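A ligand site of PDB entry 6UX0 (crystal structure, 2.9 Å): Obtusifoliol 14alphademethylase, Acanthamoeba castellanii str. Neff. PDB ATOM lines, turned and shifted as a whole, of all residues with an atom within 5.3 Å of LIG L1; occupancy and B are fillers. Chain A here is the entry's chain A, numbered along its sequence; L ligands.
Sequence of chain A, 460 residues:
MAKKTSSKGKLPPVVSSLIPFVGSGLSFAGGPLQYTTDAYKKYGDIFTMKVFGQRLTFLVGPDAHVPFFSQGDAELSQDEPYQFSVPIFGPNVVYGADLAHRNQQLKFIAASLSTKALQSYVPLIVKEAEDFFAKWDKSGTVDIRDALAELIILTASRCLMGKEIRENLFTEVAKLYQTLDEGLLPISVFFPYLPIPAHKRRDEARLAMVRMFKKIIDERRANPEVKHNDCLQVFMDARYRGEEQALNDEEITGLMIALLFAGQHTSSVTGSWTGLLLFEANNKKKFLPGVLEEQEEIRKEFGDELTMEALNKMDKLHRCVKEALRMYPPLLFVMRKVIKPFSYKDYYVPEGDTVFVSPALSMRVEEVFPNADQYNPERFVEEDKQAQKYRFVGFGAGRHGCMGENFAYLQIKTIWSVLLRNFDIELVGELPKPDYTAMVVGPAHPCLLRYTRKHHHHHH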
ATOM      1  N   TYR A  82       4.661  29.992  13.668  1.00  0.00           N
ATOM      2  CA  TYR A  82       4.835  29.397  12.330  1.00  0.00           C
ATOM      3  C   TYR A  82       6.073  29.861  11.573  1.00  0.00           C
ATOM      4  O   TYR A  82       6.216  29.576  10.384  1.00  0.00           O
ATOM      5  CB  TYR A  82       3.581  29.670  11.485  1.00  0.00           C
ATOM      6  CG  TYR A  82       2.299  28.991  11.984  1.00  0.00           C
ATOM      7  CD1 TYR A  82       2.329  27.732  12.593  1.00  0.00           C
ATOM      8  CD2 TYR A  82       1.059  29.597  11.784  1.00  0.00           C
ATOM      9  CE1 TYR A  82       1.167  27.127  13.042  1.00  0.00           C
ATOM     10  CE2 TYR A  82      -0.095  28.959  12.213  1.00  0.00           C
ATOM     11  CZ  TYR A  82      -0.012  27.736  12.844  1.00  0.00           C
ATOM     12  OH  TYR A  82      -1.090  27.101  13.301  1.00  0.00           O
ATOM     13  N   PHE A  84       8.887  28.794  11.345  1.00  0.00           N
ATOM     14  CA  PHE A  84       9.643  27.668  10.786  1.00  0.00           C
ATOM     15  C   PHE A  84       9.568  27.466   9.283  1.00  0.00           C
ATOM     16  O   PHE A  84      10.436  26.804   8.699  1.00  0.00           O
ATOM     17  CB  PHE A  84       9.119  26.373  11.387  1.00  0.00           C
ATOM     18  CG  PHE A  84       7.843  25.900  10.776  1.00  0.00           C
ATOM     19  CD1 PHE A  84       7.861  25.039   9.670  1.00  0.00           C
ATOM     20  CD2 PHE A  84       6.625  26.318  11.292  1.00  0.00           C
ATOM     21  CE1 PHE A  84       6.687  24.595   9.096  1.00  0.00           C
ATOM     22  CE2 PHE A  84       5.440  25.867  10.724  1.00  0.00           C
ATOM     23  CZ  PHE A  84       5.465  25.002   9.629  1.00  0.00           C
ATOM     24  N   PHE A  89       9.105  28.592   2.405  1.00  0.00           N
ATOM     25  CA  PHE A  89       8.208  29.277   1.413  1.00  0.00           C
ATOM     26  C   PHE A  89       8.870  30.467   0.769  1.00  0.00           C
ATOM     27  O   PHE A  89       8.845  30.660  -0.453  1.00  0.00           O
ATOM     28  CB  PHE A  89       6.923  29.849   2.042  1.00  0.00           C
ATOM     29  CG  PHE A  89       6.030  28.841   2.701  1.00  0.00           C
ATOM     30  CD1 PHE A  89       6.201  27.460   2.542  1.00  0.00           C
ATOM     31  CD2 PHE A  89       4.973  29.303   3.494  1.00  0.00           C
ATOM     32  CE1 PHE A  89       5.371  26.575   3.185  1.00  0.00           C
ATOM     33  CE2 PHE A  89       4.126  28.421   4.124  1.00  0.00           C
ATOM     34  CZ  PHE A  89       4.317  27.061   3.958  1.00  0.00           C
ATOM     35  N   VAL A  94       3.626  34.856   3.115  1.00  0.00           N
ATOM     36  CA  VAL A  94       2.691  34.293   4.070  1.00  0.00           C
ATOM     37  C   VAL A  94       3.057  34.839   5.429  1.00  0.00           C
ATOM     38  O   VAL A  94       2.683  35.966   5.758  1.00  0.00           O
ATOM     39  CB  VAL A  94       2.630  32.721   4.045  1.00  0.00           C
ATOM     40  CG1 VAL A  94       1.420  32.242   4.858  1.00  0.00           C
ATOM     41  CG2 VAL A  94       2.539  32.161   2.632  1.00  0.00           C
ATOM     42  N   TYR A  95       3.823  34.025   6.178  1.00  0.00           N
ATOM     43  CA  TYR A  95       4.231  34.296   7.535  1.00  0.00           C
ATOM     44  C   TYR A  95       5.535  35.097   7.459  1.00  0.00           C
ATOM     45  O   TYR A  95       5.860  35.856   8.368  1.00  0.00           O
ATOM     46  CB  TYR A  95       4.275  32.970   8.320  1.00  0.00           C
ATOM     47  CG  TYR A  95       2.883  32.334   8.342  1.00  0.00           C
ATOM     48  CD1 TYR A  95       1.766  33.036   8.869  1.00  0.00           C
ATOM     49  CD2 TYR A  95       2.655  31.074   7.788  1.00  0.00           C
ATOM     50  CE1 TYR A  95       0.479  32.471   8.861  1.00  0.00           C
ATOM     51  CE2 TYR A  95       1.364  30.510   7.755  1.00  0.00           C
ATOM     52  CZ  TYR A  95       0.266  31.201   8.291  1.00  0.00           C
ATOM     53  OH  TYR A  95      -1.012  30.616   8.259  1.00  0.00           O
ATOM     54  N   LEU A 106      -3.142  35.920   1.529  1.00  0.00           N
ATOM     55  CA  LEU A 106      -4.196  34.982   1.901  1.00  0.00           C
ATOM     56  C   LEU A 106      -5.349  35.140   0.915  1.00  0.00           C
ATOM     57  O   LEU A 106      -5.837  34.140   0.373  1.00  0.00           O
ATOM     58  CB  LEU A 106      -4.700  35.260   3.320  1.00  0.00           C
ATOM     59  CG  LEU A 106      -3.727  35.011   4.478  1.00  0.00           C
ATOM     60  CD1 LEU A 106      -4.402  35.355   5.810  1.00  0.00           C
ATOM     61  CD2 LEU A 106      -3.225  33.569   4.426  1.00  0.00           C
ATOM     62  N   VAL A 189      12.141  24.149  13.599  1.00  0.00           N
ATOM     63  CA  VAL A 189      10.993  24.908  14.098  1.00  0.00           C
ATOM     64  C   VAL A 189      11.319  25.971  15.159  1.00  0.00           C
ATOM     65  O   VAL A 189      10.421  26.759  15.482  1.00  0.00           O
ATOM     66  CB  VAL A 189       9.857  23.978  14.581  1.00  0.00           C
ATOM     67  CG1 VAL A 189       9.662  22.801  13.627  1.00  0.00           C
ATOM     68  CG2 VAL A 189      10.078  23.480  16.016  1.00  0.00           C
ATOM     69  N   ALA A 258       3.870  27.109  -0.973  1.00  0.00           N
ATOM     70  CA  ALA A 258       3.057  27.011   0.238  1.00  0.00           C
ATOM     71  C   ALA A 258       1.857  26.091   0.001  1.00  0.00           C
ATOM     72  O   ALA A 258       1.629  25.144   0.754  1.00  0.00           O
ATOM     73  CB  ALA A 258       2.609  28.399   0.699  1.00  0.00           C
ATOM     74  N   LEU A 259       1.132  26.358  -1.075  1.00  0.00           N
ATOM     75  CA  LEU A 259      -0.027  25.564  -1.402  1.00  0.00           C
ATOM     76  C   LEU A 259       0.374  24.126  -1.821  1.00  0.00           C
ATOM     77  O   LEU A 259      -0.411  23.204  -1.654  1.00  0.00           O
ATOM     78  CB  LEU A 259      -0.871  26.302  -2.458  1.00  0.00           C
ATOM     79  CG  LEU A 259      -1.339  27.719  -2.054  1.00  0.00           C
ATOM     80  CD1 LEU A 259      -2.526  28.237  -2.858  1.00  0.00           C
ATOM     81  CD2 LEU A 259      -1.683  27.823  -0.574  1.00  0.00           C
ATOM     82  N   PHE A 261       2.986  22.692  -0.283  1.00  0.00           N
ATOM     83  CA  PHE A 261       3.222  22.229   1.081  1.00  0.00           C
ATOM     84  C   PHE A 261       1.906  21.800   1.725  1.00  0.00           C
ATOM     85  O   PHE A 261       1.689  20.605   1.942  1.00  0.00           O
ATOM     86  CB  PHE A 261       3.906  23.341   1.902  1.00  0.00           C
ATOM     87  CG  PHE A 261       4.865  22.836   2.939  1.00  0.00           C
ATOM     88  CD1 PHE A 261       6.162  22.493   2.572  1.00  0.00           C
ATOM     89  CD2 PHE A 261       4.484  22.753   4.277  1.00  0.00           C
ATOM     90  CE1 PHE A 261       7.053  22.046   3.525  1.00  0.00           C
ATOM     91  CE2 PHE A 261       5.374  22.314   5.235  1.00  0.00           C
ATOM     92  CZ  PHE A 261       6.656  21.952   4.852  1.00  0.00           C
ATOM     93  N   ALA A 262       0.995  22.748   1.957  1.00  0.00           N
ATOM     94  CA  ALA A 262      -0.300  22.426   2.554  1.00  0.00           C
ATOM     95  C   ALA A 262      -1.012  21.199   1.930  1.00  0.00           C
ATOM     96  O   ALA A 262      -1.560  20.369   2.626  1.00  0.00           O
ATOM     97  CB  ALA A 262      -1.200  23.637   2.475  1.00  0.00           C
ATOM     98  N   GLY A 263      -0.967  21.089   0.607  1.00  0.00           N
ATOM     99  CA  GLY A 263      -1.501  19.913  -0.083  1.00  0.00           C
ATOM    100  C   GLY A 263      -0.844  18.632   0.363  1.00  0.00           C
ATOM    101  O   GLY A 263      -1.538  17.702   0.822  1.00  0.00           O
ATOM    102  N   HIS A 265       1.275  17.832   2.855  1.00  0.00           N
ATOM    103  CA  HIS A 265       1.231  17.528   4.269  1.00  0.00           C
ATOM    104  C   HIS A 265      -0.159  17.116   4.753  1.00  0.00           C
ATOM    105  O   HIS A 265      -0.248  16.455   5.768  1.00  0.00           O
ATOM    106  CB  HIS A 265       1.774  18.717   5.078  1.00  0.00           C
ATOM    107  CG  HIS A 265       3.268  18.775   5.144  1.00  0.00           C
ATOM    108  ND1 HIS A 265       4.102  18.061   4.314  1.00  0.00           N
ATOM    109  CD2 HIS A 265       4.079  19.492   5.961  1.00  0.00           C
ATOM    110  CE1 HIS A 265       5.354  18.331   4.618  1.00  0.00           C
ATOM    111  NE2 HIS A 265       5.375  19.197   5.613  1.00  0.00           N
ATOM    112  N   THR A 266      -1.234  17.429   4.041  1.00  0.00           N
ATOM    113  CA  THR A 266      -2.568  17.051   4.534  1.00  0.00           C
ATOM    114  C   THR A 266      -3.411  16.146   3.600  1.00  0.00           C
ATOM    115  O   THR A 266      -3.448  14.929   3.812  1.00  0.00           O
ATOM    116  CB  THR A 266      -3.340  18.287   4.907  1.00  0.00           C
ATOM    117  OG1 THR A 266      -3.549  19.032   3.722  1.00  0.00           O
ATOM    118  CG2 THR A 266      -2.535  19.110   5.902  1.00  0.00           C
ATOM    119  N   LEU A 331      -2.584  17.600  10.713  1.00  0.00           N
ATOM    120  CA  LEU A 331      -1.953  18.546  11.646  1.00  0.00           C
ATOM    121  C   LEU A 331      -2.357  18.126  13.014  1.00  0.00           C
ATOM    122  O   LEU A 331      -3.542  17.957  13.247  1.00  0.00           O
ATOM    123  CB  LEU A 331      -2.501  19.943  11.453  1.00  0.00           C
ATOM    124  CG  LEU A 331      -2.170  20.577  10.116  1.00  0.00           C
ATOM    125  CD1 LEU A 331      -3.198  21.673   9.853  1.00  0.00           C
ATOM    126  CD2 LEU A 331      -0.729  21.080  10.076  1.00  0.00           C
ATOM    127  N   PHE A 333      -1.724  19.835  15.936  1.00  0.00           N
ATOM    128  CA  PHE A 333      -2.210  21.008  16.637  1.00  0.00           C
ATOM    129  C   PHE A 333      -1.868  22.314  15.935  1.00  0.00           C
ATOM    130  O   PHE A 333      -0.936  22.386  15.118  1.00  0.00           O
ATOM    131  CB  PHE A 333      -1.673  21.035  18.075  1.00  0.00           C
ATOM    132  CG  PHE A 333      -0.242  20.606  18.186  1.00  0.00           C
ATOM    133  CD1 PHE A 333       0.784  21.414  17.699  1.00  0.00           C
ATOM    134  CD2 PHE A 333       0.083  19.383  18.765  1.00  0.00           C
ATOM    135  CE1 PHE A 333       2.109  21.020  17.763  1.00  0.00           C
ATOM    136  CE2 PHE A 333       1.399  18.974  18.831  1.00  0.00           C
ATOM    137  CZ  PHE A 333       2.414  19.795  18.338  1.00  0.00           C
ATOM    138  N   VAL A 334      -2.589  23.356  16.313  1.00  0.00           N
ATOM    139  CA  VAL A 334      -2.461  24.682  15.705  1.00  0.00           C
ATOM    140  C   VAL A 334      -2.178  25.757  16.766  1.00  0.00           C
ATOM    141  O   VAL A 334      -2.778  25.739  17.839  1.00  0.00           O
ATOM    142  CB  VAL A 334      -3.712  25.028  14.860  1.00  0.00           C
ATOM    143  CG1 VAL A 334      -3.755  24.168  13.586  1.00  0.00           C
ATOM    144  CG2 VAL A 334      -5.003  24.861  15.657  1.00  0.00           C
ATOM    145  N   MET A 335      -1.277  26.696  16.462  1.00  0.00           N
ATOM    146  CA  MET A 335      -0.647  27.559  17.473  1.00  0.00           C
ATOM    147  C   MET A 335      -0.737  29.058  17.156  1.00  0.00           C
ATOM    148  O   MET A 335      -0.813  29.460  16.001  1.00  0.00           O
ATOM    149  CB  MET A 335       0.844  27.205  17.644  1.00  0.00           C
ATOM    150  CG  MET A 335       1.248  25.763  17.332  1.00  0.00           C
ATOM    151  SD  MET A 335       3.050  25.536  17.330  1.00  0.00           S
ATOM    152  CE  MET A 335       3.508  26.369  15.820  1.00  0.00           C
ATOM    153  N   CYS A 402      -9.115  26.934   7.075  1.00  0.00           N
ATOM    154  CA  CYS A 402      -8.483  26.406   5.868  1.00  0.00           C
ATOM    155  C   CYS A 402      -9.092  26.930   4.595  1.00  0.00           C
ATOM    156  O   CYS A 402     -10.254  26.605   4.284  1.00  0.00           O
ATOM    157  CB  CYS A 402      -8.523  24.861   5.828  1.00  0.00           C
ATOM    158  SG  CYS A 402      -7.475  24.084   4.561  1.00  0.00           S
ATOM    159  N   MET A 439       7.462  14.683  10.820  1.00  0.00           N
ATOM    160  CA  MET A 439       6.783  15.982  10.890  1.00  0.00           C
ATOM    161  C   MET A 439       5.352  15.871  10.365  1.00  0.00           C
ATOM    162  O   MET A 439       4.414  16.453  10.932  1.00  0.00           O
ATOM    163  CB  MET A 439       7.567  17.002  10.085  1.00  0.00           C
ATOM    164  CG  MET A 439       8.835  17.482  10.760  1.00  0.00           C
ATOM    165  SD  MET A 439       8.573  18.331  12.332  1.00  0.00           S
ATOM    166  CE  MET A 439       7.054  19.259  12.072  1.00  0.00           C
HETATM  167  C1  LIG L   1       1.003  27.166   9.102  1.00  0.00           C
HETATM  168  C2  LIG L   1       0.992  25.689   8.725  1.00  0.00           C
HETATM  169  C3  LIG L   1       0.894  24.912  10.025  1.00  0.00           C
HETATM  170  N1  LIG L   1       1.874  24.181  10.555  1.00  0.00           N
HETATM  171  C4  LIG L   1       1.369  23.589  11.826  1.00  0.00           C
HETATM  172  C5  LIG L   1       0.090  23.927  12.170  1.00  0.00           C
HETATM  173  S1  LIG L   1      -0.581  24.944  10.967  1.00  0.00           S
HETATM  174  C6  LIG L   1       2.317  22.792  12.549  1.00  0.00           C
HETATM  175  C7  LIG L   1       2.626  23.253  13.805  1.00  0.00           C
HETATM  176  C8  LIG L   1       3.541  22.586  14.558  1.00  0.00           C
HETATM  177  C9  LIG L   1       4.088  21.459  14.007  1.00  0.00           C
HETATM  178  C10 LIG L   1       3.790  20.971  12.759  1.00  0.00           C
HETATM  179  C11 LIG L   1       2.895  21.660  12.000  1.00  0.00           C
HETATM  180  C12 LIG L   1       5.031  20.804  14.809  1.00  0.00           C
HETATM  181  N2  LIG L   1       5.783  20.359  15.579  1.00  0.00           N
HETATM  182  C13 LIG L   1      -0.133  25.430   7.726  1.00  0.00           C
HETATM  183  C14 LIG L   1      -0.399  23.926   7.500  1.00  0.00           C
HETATM  184  N3  LIG L   1      -1.465  23.487   6.588  1.00  0.00           N
HETATM  185  C15 LIG L   1      -2.675  24.066   6.327  1.00  0.00           C
HETATM  186  N4  LIG L   1      -3.396  23.354   5.482  1.00  0.00           N
HETATM  187  C16 LIG L   1      -2.558  22.315   5.250  1.00  0.00           C
HETATM  188  N5  LIG L   1      -1.379  22.328   5.905  1.00  0.00           N
HETATM  189  C17 LIG L   1       0.009  26.104   6.379  1.00  0.00           C
HETATM  190  C18 LIG L   1       0.757  25.607   5.310  1.00  0.00           C
HETATM  191  C19 LIG L   1       0.823  26.243   4.070  1.00  0.00           C
HETATM  192  C20 LIG L   1       0.132  27.407   3.843  1.00  0.00           C
HETATM  193  C21 LIG L   1      -0.629  27.905   4.884  1.00  0.00           C
HETATM  194  C22 LIG L   1      -0.673  27.281   6.114  1.00  0.00           C
HETATM  195  F1  LIG L   1      -1.349  29.032   4.785  1.00  0.00           F
HETATM  196  F2  LIG L   1       1.459  24.480   5.479  1.00  0.00           F
HETATM  197  O1  LIG L   1      -1.249  25.978   8.431  1.00  0.00           O
HETATM  198  C1  LG2 L   2      -5.287  26.609   7.077  1.00  0.00           C
HETATM  199  C2  LG2 L   2      -6.326  21.947   7.747  1.00  0.00           C
HETATM  200  C3  LG2 L   2      -5.540  21.220   3.073  1.00  0.00           C
HETATM  201  C4  LG2 L   2      -4.441  25.866   2.416  1.00  0.00           C
HETATM  202  C5  LG2 L   2      -5.652  25.418   7.656  1.00  0.00           C
HETATM  203  C6  LG2 L   2      -5.918  25.214   9.045  1.00  0.00           C
HETATM  204  C7  LG2 L   2      -6.209  23.878   9.204  1.00  0.00           C
HETATM  205  C8  LG2 L   2      -6.128  23.282   7.945  1.00  0.00           C
HETATM  206  C9  LG2 L   2      -6.565  23.141  10.482  1.00  0.00           C
HETATM  207  C10 LG2 L   2      -5.882  26.258  10.148  1.00  0.00           C
HETATM  208  C11 LG2 L   2      -4.432  26.389  10.629  1.00  0.00           C
HETATM  209  C12 LG2 L   2      -4.230  27.541  11.568  1.00  0.00           C
HETATM  210  O1  LG2 L   2      -3.171  28.222  11.524  1.00  0.00           O
HETATM  211  O2  LG2 L   2      -5.133  27.811  12.409  1.00  0.00           O
HETATM  212  C13 LG2 L   2      -6.186  21.349   6.498  1.00  0.00           C
HETATM  213  C14 LG2 L   2      -6.454  19.982   6.302  1.00  0.00           C
HETATM  214  C15 LG2 L   2      -6.238  19.721   4.985  1.00  0.00           C
HETATM  215  C16 LG2 L   2      -5.845  21.029   4.404  1.00  0.00           C
HETATM  216  C17 LG2 L   2      -6.886  19.034   7.402  1.00  0.00           C
HETATM  217  C18 LG2 L   2      -6.430  18.475   4.168  1.00  0.00           C
HETATM  218  C19 LG2 L   2      -7.182  17.441   4.535  1.00  0.00           C
HETATM  219  C20 LG2 L   2      -5.177  22.409   2.457  1.00  0.00           C
HETATM  220  C21 LG2 L   2      -4.836  22.565   1.122  1.00  0.00           C
HETATM  221  C22 LG2 L   2      -4.523  23.912   0.914  1.00  0.00           C
HETATM  222  C23 LG2 L   2      -4.678  24.539   2.167  1.00  0.00           C
HETATM  223  C24 LG2 L   2      -4.821  21.453   0.093  1.00  0.00           C
HETATM  224  C25 LG2 L   2      -4.096  24.635  -0.311  1.00  0.00           C
HETATM  225  C26 LG2 L   2      -3.970  24.115  -1.535  1.00  0.00           C
HETATM  226  C27 LG2 L   2      -4.590  26.416   3.681  1.00  0.00           C
HETATM  227  C28 LG2 L   2      -4.331  27.849   3.882  1.00  0.00           C
HETATM  228  C29 LG2 L   2      -4.597  28.079   5.169  1.00  0.00           C
HETATM  229  C30 LG2 L   2      -4.977  26.756   5.743  1.00  0.00           C
HETATM  230  C31 LG2 L   2      -3.900  28.891   2.867  1.00  0.00           C
HETATM  231  C32 LG2 L   2      -4.384  29.415   5.867  1.00  0.00           C
HETATM  232  C33 LG2 L   2      -5.500  30.379   6.239  1.00  0.00           C
HETATM  233  C34 LG2 L   2      -4.889  31.547   7.036  1.00  0.00           C
HETATM  234  O3  LG2 L   2      -3.762  31.541   7.620  1.00  0.00           O
HETATM  235  O4  LG2 L   2      -5.529  32.628   7.127  1.00  0.00           O
HETATM  236  N1  LG2 L   2      -5.737  24.216   7.009  1.00  0.00           N
HETATM  237  N2  LG2 L   2      -5.827  21.916   5.363  1.00  0.00           N
HETATM  238  N3  LG2 L   2      -5.041  23.593   3.077  1.00  0.00           N
HETATM  239  N4  LG2 L   2      -4.963  25.784   4.818  1.00  0.00           N
HETATM  240 FE1  LG2 L   2      -5.372  23.930   5.087  1.00  0.00          FE
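An iron atom (FE1) of LG2 L2 is bound by a nitrogen (N4) of LIG L1 (2.1 Å).
The side-chain hydroxyl of Tyr 82 sits at hydrogen-bond distance from an oxygen (O1) of LG2 L2 (3.0 Å).
OH of Tyr 95 sits at hydrogen-bond distance from O3 of LG2 L2, at 3.0 Å.
The side-chain hydroxyl of Tyr 82 lies close to a sulfur (S1) of LIG L1, 3.2 Å away.
FE1 of LG2 L2 is bound by SG of Cys 402.
Residues that only touch LIG L1: Thr 266 (3.3 Å), Ala 262 (3.4 Å), Phe 333 (3.5 Å), Ala 258 (3.6 Å), Phe 89 (3.6 Å), Tyr 95 (3.6 Å), Leu 331 (3.6 Å), Phe 261 (3.7 Å), Met 439 (3.7 Å), Phe 84 (3.8 Å) and Met 335 (3.8 Å).
Hydrophobic or aromatic side chains that line LIG L1: Tyr 82, Phe 84, Phe 89, Tyr 95, Phe 261, Ala 262, Leu 331, Phe 333, Met 335 and Met 439.
Along chain A the residues within 4 Å of LIG L1 span positions 82 to 439.
The backbone NH (N) of Met 335 is in hydrogen-bond range of the side-chain hydroxyl (OH) of Tyr 82, 3.2 Å away.
The backbone carbonyl oxygen of Ala 262 lies within hydrogen-bond range of the side-chain hydroxyl of Thr 266, 2.6 Å away.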
